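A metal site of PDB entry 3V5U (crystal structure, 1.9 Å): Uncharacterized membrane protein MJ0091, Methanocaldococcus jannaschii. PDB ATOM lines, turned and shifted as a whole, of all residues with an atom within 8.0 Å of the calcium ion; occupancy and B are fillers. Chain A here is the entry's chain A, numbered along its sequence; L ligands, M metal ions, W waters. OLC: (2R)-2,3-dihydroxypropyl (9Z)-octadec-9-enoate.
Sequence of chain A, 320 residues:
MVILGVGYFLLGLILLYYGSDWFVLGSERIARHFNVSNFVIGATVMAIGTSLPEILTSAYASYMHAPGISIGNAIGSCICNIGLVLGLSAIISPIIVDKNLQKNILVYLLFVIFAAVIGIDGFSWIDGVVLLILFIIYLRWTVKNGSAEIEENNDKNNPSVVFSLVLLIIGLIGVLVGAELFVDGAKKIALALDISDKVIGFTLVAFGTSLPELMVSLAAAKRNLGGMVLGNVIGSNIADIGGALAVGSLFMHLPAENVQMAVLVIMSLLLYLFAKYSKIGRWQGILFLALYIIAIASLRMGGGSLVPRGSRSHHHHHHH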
ATOM      1  N   ALA A 115     -11.911 -10.754 -18.556  1.00  0.00           N
ATOM      2  CA  ALA A 115     -10.844 -11.732 -18.812  1.00  0.00           C
ATOM      3  C   ALA A 115     -10.173 -11.503 -20.163  1.00  0.00           C
ATOM      4  O   ALA A 115      -8.933 -11.544 -20.275  1.00  0.00           O
ATOM      5  CB  ALA A 115     -11.404 -13.144 -18.736  1.00  0.00           C
ATOM      6  N   ALA A 116     -10.974 -11.264 -21.191  1.00  0.00           N
ATOM      7  CA  ALA A 116     -10.429 -11.085 -22.540  1.00  0.00           C
ATOM      8  C   ALA A 116      -9.475  -9.889 -22.571  1.00  0.00           C
ATOM      9  O   ALA A 116      -8.386  -9.950 -23.153  1.00  0.00           O
ATOM     10  CB  ALA A 116     -11.532 -10.924 -23.568  1.00  0.00           C
ATOM     11  N   VAL A 117      -9.885  -8.802 -21.926  1.00  0.00           N
ATOM     12  CA  VAL A 117      -9.104  -7.570 -21.917  1.00  0.00           C
ATOM     13  C   VAL A 117      -7.783  -7.753 -21.158  1.00  0.00           C
ATOM     14  O   VAL A 117      -6.703  -7.462 -21.684  1.00  0.00           O
ATOM     15  CB  VAL A 117      -9.918  -6.399 -21.297  1.00  0.00           C
ATOM     16  CG1 VAL A 117      -9.010  -5.214 -20.988  1.00  0.00           C
ATOM     17  CG2 VAL A 117     -11.026  -5.991 -22.247  1.00  0.00           C
ATOM     18  N   ILE A 118      -7.845  -8.218 -19.923  1.00  0.00           N
ATOM     19  CA  ILE A 118      -6.597  -8.390 -19.180  1.00  0.00           C
ATOM     20  C   ILE A 118      -5.745  -9.494 -19.793  1.00  0.00           C
ATOM     21  O   ILE A 118      -4.549  -9.549 -19.551  1.00  0.00           O
ATOM     22  CB  ILE A 118      -6.789  -8.662 -17.676  1.00  0.00           C
ATOM     23  CG1 ILE A 118      -7.297 -10.086 -17.407  1.00  0.00           C
ATOM     24  CG2 ILE A 118      -7.664  -7.571 -17.012  1.00  0.00           C
ATOM     25  CD1 ILE A 118      -7.423 -10.401 -15.913  1.00  0.00           C
ATOM     26  N   GLY A 119      -6.340 -10.345 -20.614  1.00  0.00           N
ATOM     27  CA  GLY A 119      -5.583 -11.408 -21.270  1.00  0.00           C
ATOM     28  C   GLY A 119      -4.912 -11.026 -22.591  1.00  0.00           C
ATOM     29  O   GLY A 119      -4.240 -11.861 -23.211  1.00  0.00           O
ATOM     30  N   ILE A 120      -5.072  -9.784 -23.037  1.00  0.00           N
ATOM     31  CA  ILE A 120      -4.541  -9.386 -24.348  1.00  0.00           C
ATOM     32  C   ILE A 120      -3.021  -9.608 -24.450  1.00  0.00           C
ATOM     33  O   ILE A 120      -2.509  -9.960 -25.513  1.00  0.00           O
ATOM     34  CB  ILE A 120      -4.910  -7.930 -24.707  1.00  0.00           C
ATOM     35  CG1 ILE A 120      -6.412  -7.817 -24.979  1.00  0.00           C
ATOM     36  CG2 ILE A 120      -4.133  -7.463 -25.925  1.00  0.00           C
ATOM     37  CD1 ILE A 120      -6.917  -6.391 -25.039  1.00  0.00           C
ATOM     38  N   ASP A 121      -2.318  -9.407 -23.343  1.00  0.00           N
ATOM     39  CA  ASP A 121      -0.866  -9.631 -23.304  1.00  0.00           C
ATOM     40  C   ASP A 121      -0.548 -10.918 -22.555  1.00  0.00           C
ATOM     41  O   ASP A 121       0.523 -11.052 -21.983  1.00  0.00           O
ATOM     42  CB  ASP A 121      -0.156  -8.430 -22.664  1.00  0.00           C
ATOM     43  CG  ASP A 121      -0.645  -8.136 -21.245  1.00  0.00           C
ATOM     44  OD1 ASP A 121      -1.706  -8.655 -20.839  1.00  0.00           O
ATOM     45  OD2 ASP A 121       0.036  -7.370 -20.533  1.00  0.00           O
ATOM     46  N   GLY A 122      -1.476 -11.870 -22.574  1.00  0.00           N
ATOM     47  CA  GLY A 122      -1.317 -13.114 -21.830  1.00  0.00           C
ATOM     48  C   GLY A 122      -1.819 -12.973 -20.402  1.00  0.00           C
ATOM     49  O   GLY A 122      -2.254 -11.925 -20.008  1.00  0.00           O
ATOM     50  N   PHE A 123      -1.771 -14.042 -19.629  1.00  0.00           N
ATOM     51  CA  PHE A 123      -2.283 -14.004 -18.264  1.00  0.00           C
ATOM     52  C   PHE A 123      -1.135 -14.248 -17.288  1.00  0.00           C
ATOM     53  O   PHE A 123      -0.469 -15.290 -17.343  1.00  0.00           O
ATOM     54  CB  PHE A 123      -3.360 -15.060 -18.078  1.00  0.00           C
ATOM     55  CG  PHE A 123      -4.616 -14.794 -18.859  1.00  0.00           C
ATOM     56  CD1 PHE A 123      -5.652 -14.049 -18.289  1.00  0.00           C
ATOM     57  CD2 PHE A 123      -4.775 -15.276 -20.146  1.00  0.00           C
ATOM     58  CE1 PHE A 123      -6.817 -13.815 -18.995  1.00  0.00           C
ATOM     59  CE2 PHE A 123      -5.952 -15.038 -20.864  1.00  0.00           C
ATOM     60  CZ  PHE A 123      -6.958 -14.305 -20.294  1.00  0.00           C
ATOM     61  N   SER A 124      -0.904 -13.292 -16.392  1.00  0.00           N
ATOM     62  CA  SER A 124       0.126 -13.441 -15.380  1.00  0.00           C
ATOM     63  C   SER A 124      -0.522 -13.994 -14.132  1.00  0.00           C
ATOM     64  O   SER A 124      -1.743 -14.193 -14.070  1.00  0.00           O
ATOM     65  CB  SER A 124       0.741 -12.089 -15.031  1.00  0.00           C
ATOM     66  OG  SER A 124      -0.220 -11.272 -14.357  1.00  0.00           O
ATOM     67  N   TRP A 125       0.306 -14.225 -13.128  1.00  0.00           N
ATOM     68  CA  TRP A 125      -0.184 -14.796 -11.893  1.00  0.00           C
ATOM     69  C   TRP A 125      -1.078 -13.799 -11.172  1.00  0.00           C
ATOM     70  O   TRP A 125      -1.992 -14.183 -10.449  1.00  0.00           O
ATOM     71  CB  TRP A 125       1.001 -15.238 -11.012  1.00  0.00           C
ATOM     72  CG  TRP A 125       1.873 -14.114 -10.579  1.00  0.00           C
ATOM     73  CD1 TRP A 125       2.973 -13.623 -11.221  1.00  0.00           C
ATOM     74  CD2 TRP A 125       1.708 -13.319  -9.394  1.00  0.00           C
ATOM     75  NE1 TRP A 125       3.509 -12.574 -10.498  1.00  0.00           N
ATOM     76  CE2 TRP A 125       2.749 -12.367  -9.376  1.00  0.00           C
ATOM     77  CE3 TRP A 125       0.783 -13.333  -8.342  1.00  0.00           C
ATOM     78  CZ2 TRP A 125       2.896 -11.446  -8.351  1.00  0.00           C
ATOM     79  CZ3 TRP A 125       0.930 -12.412  -7.316  1.00  0.00           C
ATOM     80  CH2 TRP A 125       1.973 -11.474  -7.338  1.00  0.00           C
ATOM     81  N   ILE A 126      -0.850 -12.507 -11.396  1.00  0.00           N
ATOM     82  CA  ILE A 126      -1.715 -11.483 -10.812  1.00  0.00           C
ATOM     83  C   ILE A 126      -3.081 -11.472 -11.503  1.00  0.00           C
ATOM     84  O   ILE A 126      -4.105 -11.287 -10.849  1.00  0.00           O
ATOM     85  CB  ILE A 126      -1.100 -10.059 -10.872  1.00  0.00           C
ATOM     86  CG1 ILE A 126       0.260 -10.024 -10.186  1.00  0.00           C
ATOM     87  CG2 ILE A 126      -1.999  -9.073 -10.166  1.00  0.00           C
ATOM     88  CD1 ILE A 126       0.936  -8.645 -10.278  1.00  0.00           C
ATOM     89  N   ASP A 127      -3.085 -11.666 -12.815  1.00  0.00           N
ATOM     90  CA  ASP A 127      -4.352 -11.868 -13.518  1.00  0.00           C
ATOM     91  C   ASP A 127      -5.112 -13.041 -12.893  1.00  0.00           C
ATOM     92  O   ASP A 127      -6.318 -12.962 -12.654  1.00  0.00           O
ATOM     93  CB  ASP A 127      -4.127 -12.130 -15.008  1.00  0.00           C
ATOM     94  CG  ASP A 127      -3.544 -10.923 -15.739  1.00  0.00           C
ATOM     95  OD1 ASP A 127      -3.841  -9.779 -15.369  1.00  0.00           O
ATOM     96  OD2 ASP A 127      -2.790 -11.156 -16.705  1.00  0.00           O
ATOM     97  N   GLY A 128      -4.400 -14.138 -12.638  1.00  0.00           N
ATOM     98  CA  GLY A 128      -5.004 -15.310 -12.050  1.00  0.00           C
ATOM     99  C   GLY A 128      -5.649 -15.034 -10.706  1.00  0.00           C
ATOM    100  O   GLY A 128      -6.777 -15.477 -10.436  1.00  0.00           O
ATOM    101  N   HIS A 253       3.464 -17.807 -16.811  1.00  0.00           N
ATOM    102  CA  HIS A 253       2.690 -16.855 -17.595  1.00  0.00           C
ATOM    103  C   HIS A 253       1.999 -17.606 -18.746  1.00  0.00           C
ATOM    104  O   HIS A 253       2.616 -18.428 -19.400  1.00  0.00           O
ATOM    105  CB  HIS A 253       3.607 -15.764 -18.151  1.00  0.00           C
ATOM    106  CG  HIS A 253       2.870 -14.643 -18.812  1.00  0.00           C
ATOM    107  ND1 HIS A 253       2.355 -13.573 -18.118  1.00  0.00           N
ATOM    108  CD2 HIS A 253       2.552 -14.423 -20.112  1.00  0.00           C
ATOM    109  CE1 HIS A 253       1.754 -12.749 -18.952  1.00  0.00           C
ATOM    110  NE2 HIS A 253       1.860 -13.241 -20.171  1.00  0.00           N
ATOM    111  N   LEU A 254       0.713 -17.340 -18.977  1.00  0.00           N
ATOM    112  CA  LEU A 254       0.008 -18.014 -20.067  1.00  0.00           C
ATOM    113  C   LEU A 254       0.003 -17.102 -21.286  1.00  0.00           C
ATOM    114  O   LEU A 254      -0.305 -15.924 -21.184  1.00  0.00           O
ATOM    115  CB  LEU A 254      -1.430 -18.350 -19.650  1.00  0.00           C
ATOM    116  CG  LEU A 254      -1.626 -19.096 -18.326  1.00  0.00           C
ATOM    117  CD1 LEU A 254      -3.110 -19.373 -18.087  1.00  0.00           C
ATOM    118  CD2 LEU A 254      -0.813 -20.395 -18.264  1.00  0.00           C
ATOM    119  N   ALA A 256      -1.065 -15.230 -24.721  1.00  0.00           N
ATOM    120  CA  ALA A 256      -2.357 -14.742 -25.177  1.00  0.00           C
ATOM    121  C   ALA A 256      -3.014 -15.656 -26.212  1.00  0.00           C
ATOM    122  O   ALA A 256      -2.335 -16.242 -27.054  1.00  0.00           O
ATOM    123  CB  ALA A 256      -2.234 -13.327 -25.733  1.00  0.00           C
HETATM  124  C18 OLC L   1     -19.001  -4.465 -10.569  1.00  0.00           C
HETATM  125  C10 OLC L   1     -15.354  -5.343 -17.436  1.00  0.00           C
HETATM  126  C9  OLC L   1     -14.831  -5.001 -18.830  1.00  0.00           C
HETATM  127  C17 OLC L   1     -20.040  -4.172 -11.653  1.00  0.00           C
HETATM  128  C11 OLC L   1     -15.452  -4.210 -16.413  1.00  0.00           C
HETATM  129  C8  OLC L   1     -14.433  -3.556 -19.101  1.00  0.00           C
HETATM  130  C24 OLC L   1      -3.586  -6.946 -17.647  1.00  0.00           C
HETATM  131  C16 OLC L   1     -19.876  -2.735 -12.161  1.00  0.00           C
HETATM  132  C12 OLC L   1     -16.788  -4.332 -15.685  1.00  0.00           C
HETATM  133  C7  OLC L   1     -12.917  -3.379 -19.204  1.00  0.00           C
HETATM  134  C15 OLC L   1     -18.479  -2.513 -12.761  1.00  0.00           C
HETATM  135  C13 OLC L   1     -16.931  -3.279 -14.583  1.00  0.00           C
HETATM  136  C6  OLC L   1     -12.141  -3.697 -17.918  1.00  0.00           C
HETATM  137  C14 OLC L   1     -18.288  -3.487 -13.928  1.00  0.00           C
HETATM  138  C5  OLC L   1     -10.669  -3.486 -18.306  1.00  0.00           C
HETATM  139  C4  OLC L   1      -9.647  -3.680 -17.200  1.00  0.00           C
HETATM  140  C3  OLC L   1      -8.290  -3.501 -17.897  1.00  0.00           C
HETATM  141  C2  OLC L   1      -7.108  -3.673 -16.942  1.00  0.00           C
HETATM  142  C21 OLC L   1      -3.597  -4.489 -18.074  1.00  0.00           C
HETATM  143  C1  OLC L   1      -5.800  -3.576 -17.758  1.00  0.00           C
HETATM  144  C22 OLC L   1      -2.771  -5.667 -17.518  1.00  0.00           C
HETATM  145  O19 OLC L   1      -5.703  -2.810 -18.714  1.00  0.00           O
HETATM  146  O25 OLC L   1      -2.815  -8.020 -17.113  1.00  0.00           O
HETATM  147  O23 OLC L   1      -1.534  -5.846 -18.239  1.00  0.00           O
HETATM  148  O20 OLC L   1      -4.821  -4.434 -17.321  1.00  0.00           O
HETATM  149 CA    CA M   1      -2.360  -9.875 -18.761  1.00  0.00          CA
HETATM  150  O   HOH W   1       0.122 -10.096 -18.160  1.00  0.00           O
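The backbone NH (N) of Asp 127 sits at hydrogen-bond distance from the side-chain hydroxyl (OG) of Ser 124, at 3.3 Å.
A ring nitrogen (NE2) of His 253 lies within hydrogen-bond range of the backbone carbonyl oxygen (O) of Asp 121 (3.1 Å).
Four residues have an atom within 4 Å of the calcium ion: Ile 118, Asp 121, Gly 122 and Asp 127.
The calcium ion is bound by O of Ile 118 (2.3 Å), O of Gly 122 (2.4 Å), OD2 of Asp 127 (2.5 Å), OD1 of Asp 121 (2.5 Å), O25 of the ligand (2.5 Å) and water W1 (2.6 Å).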
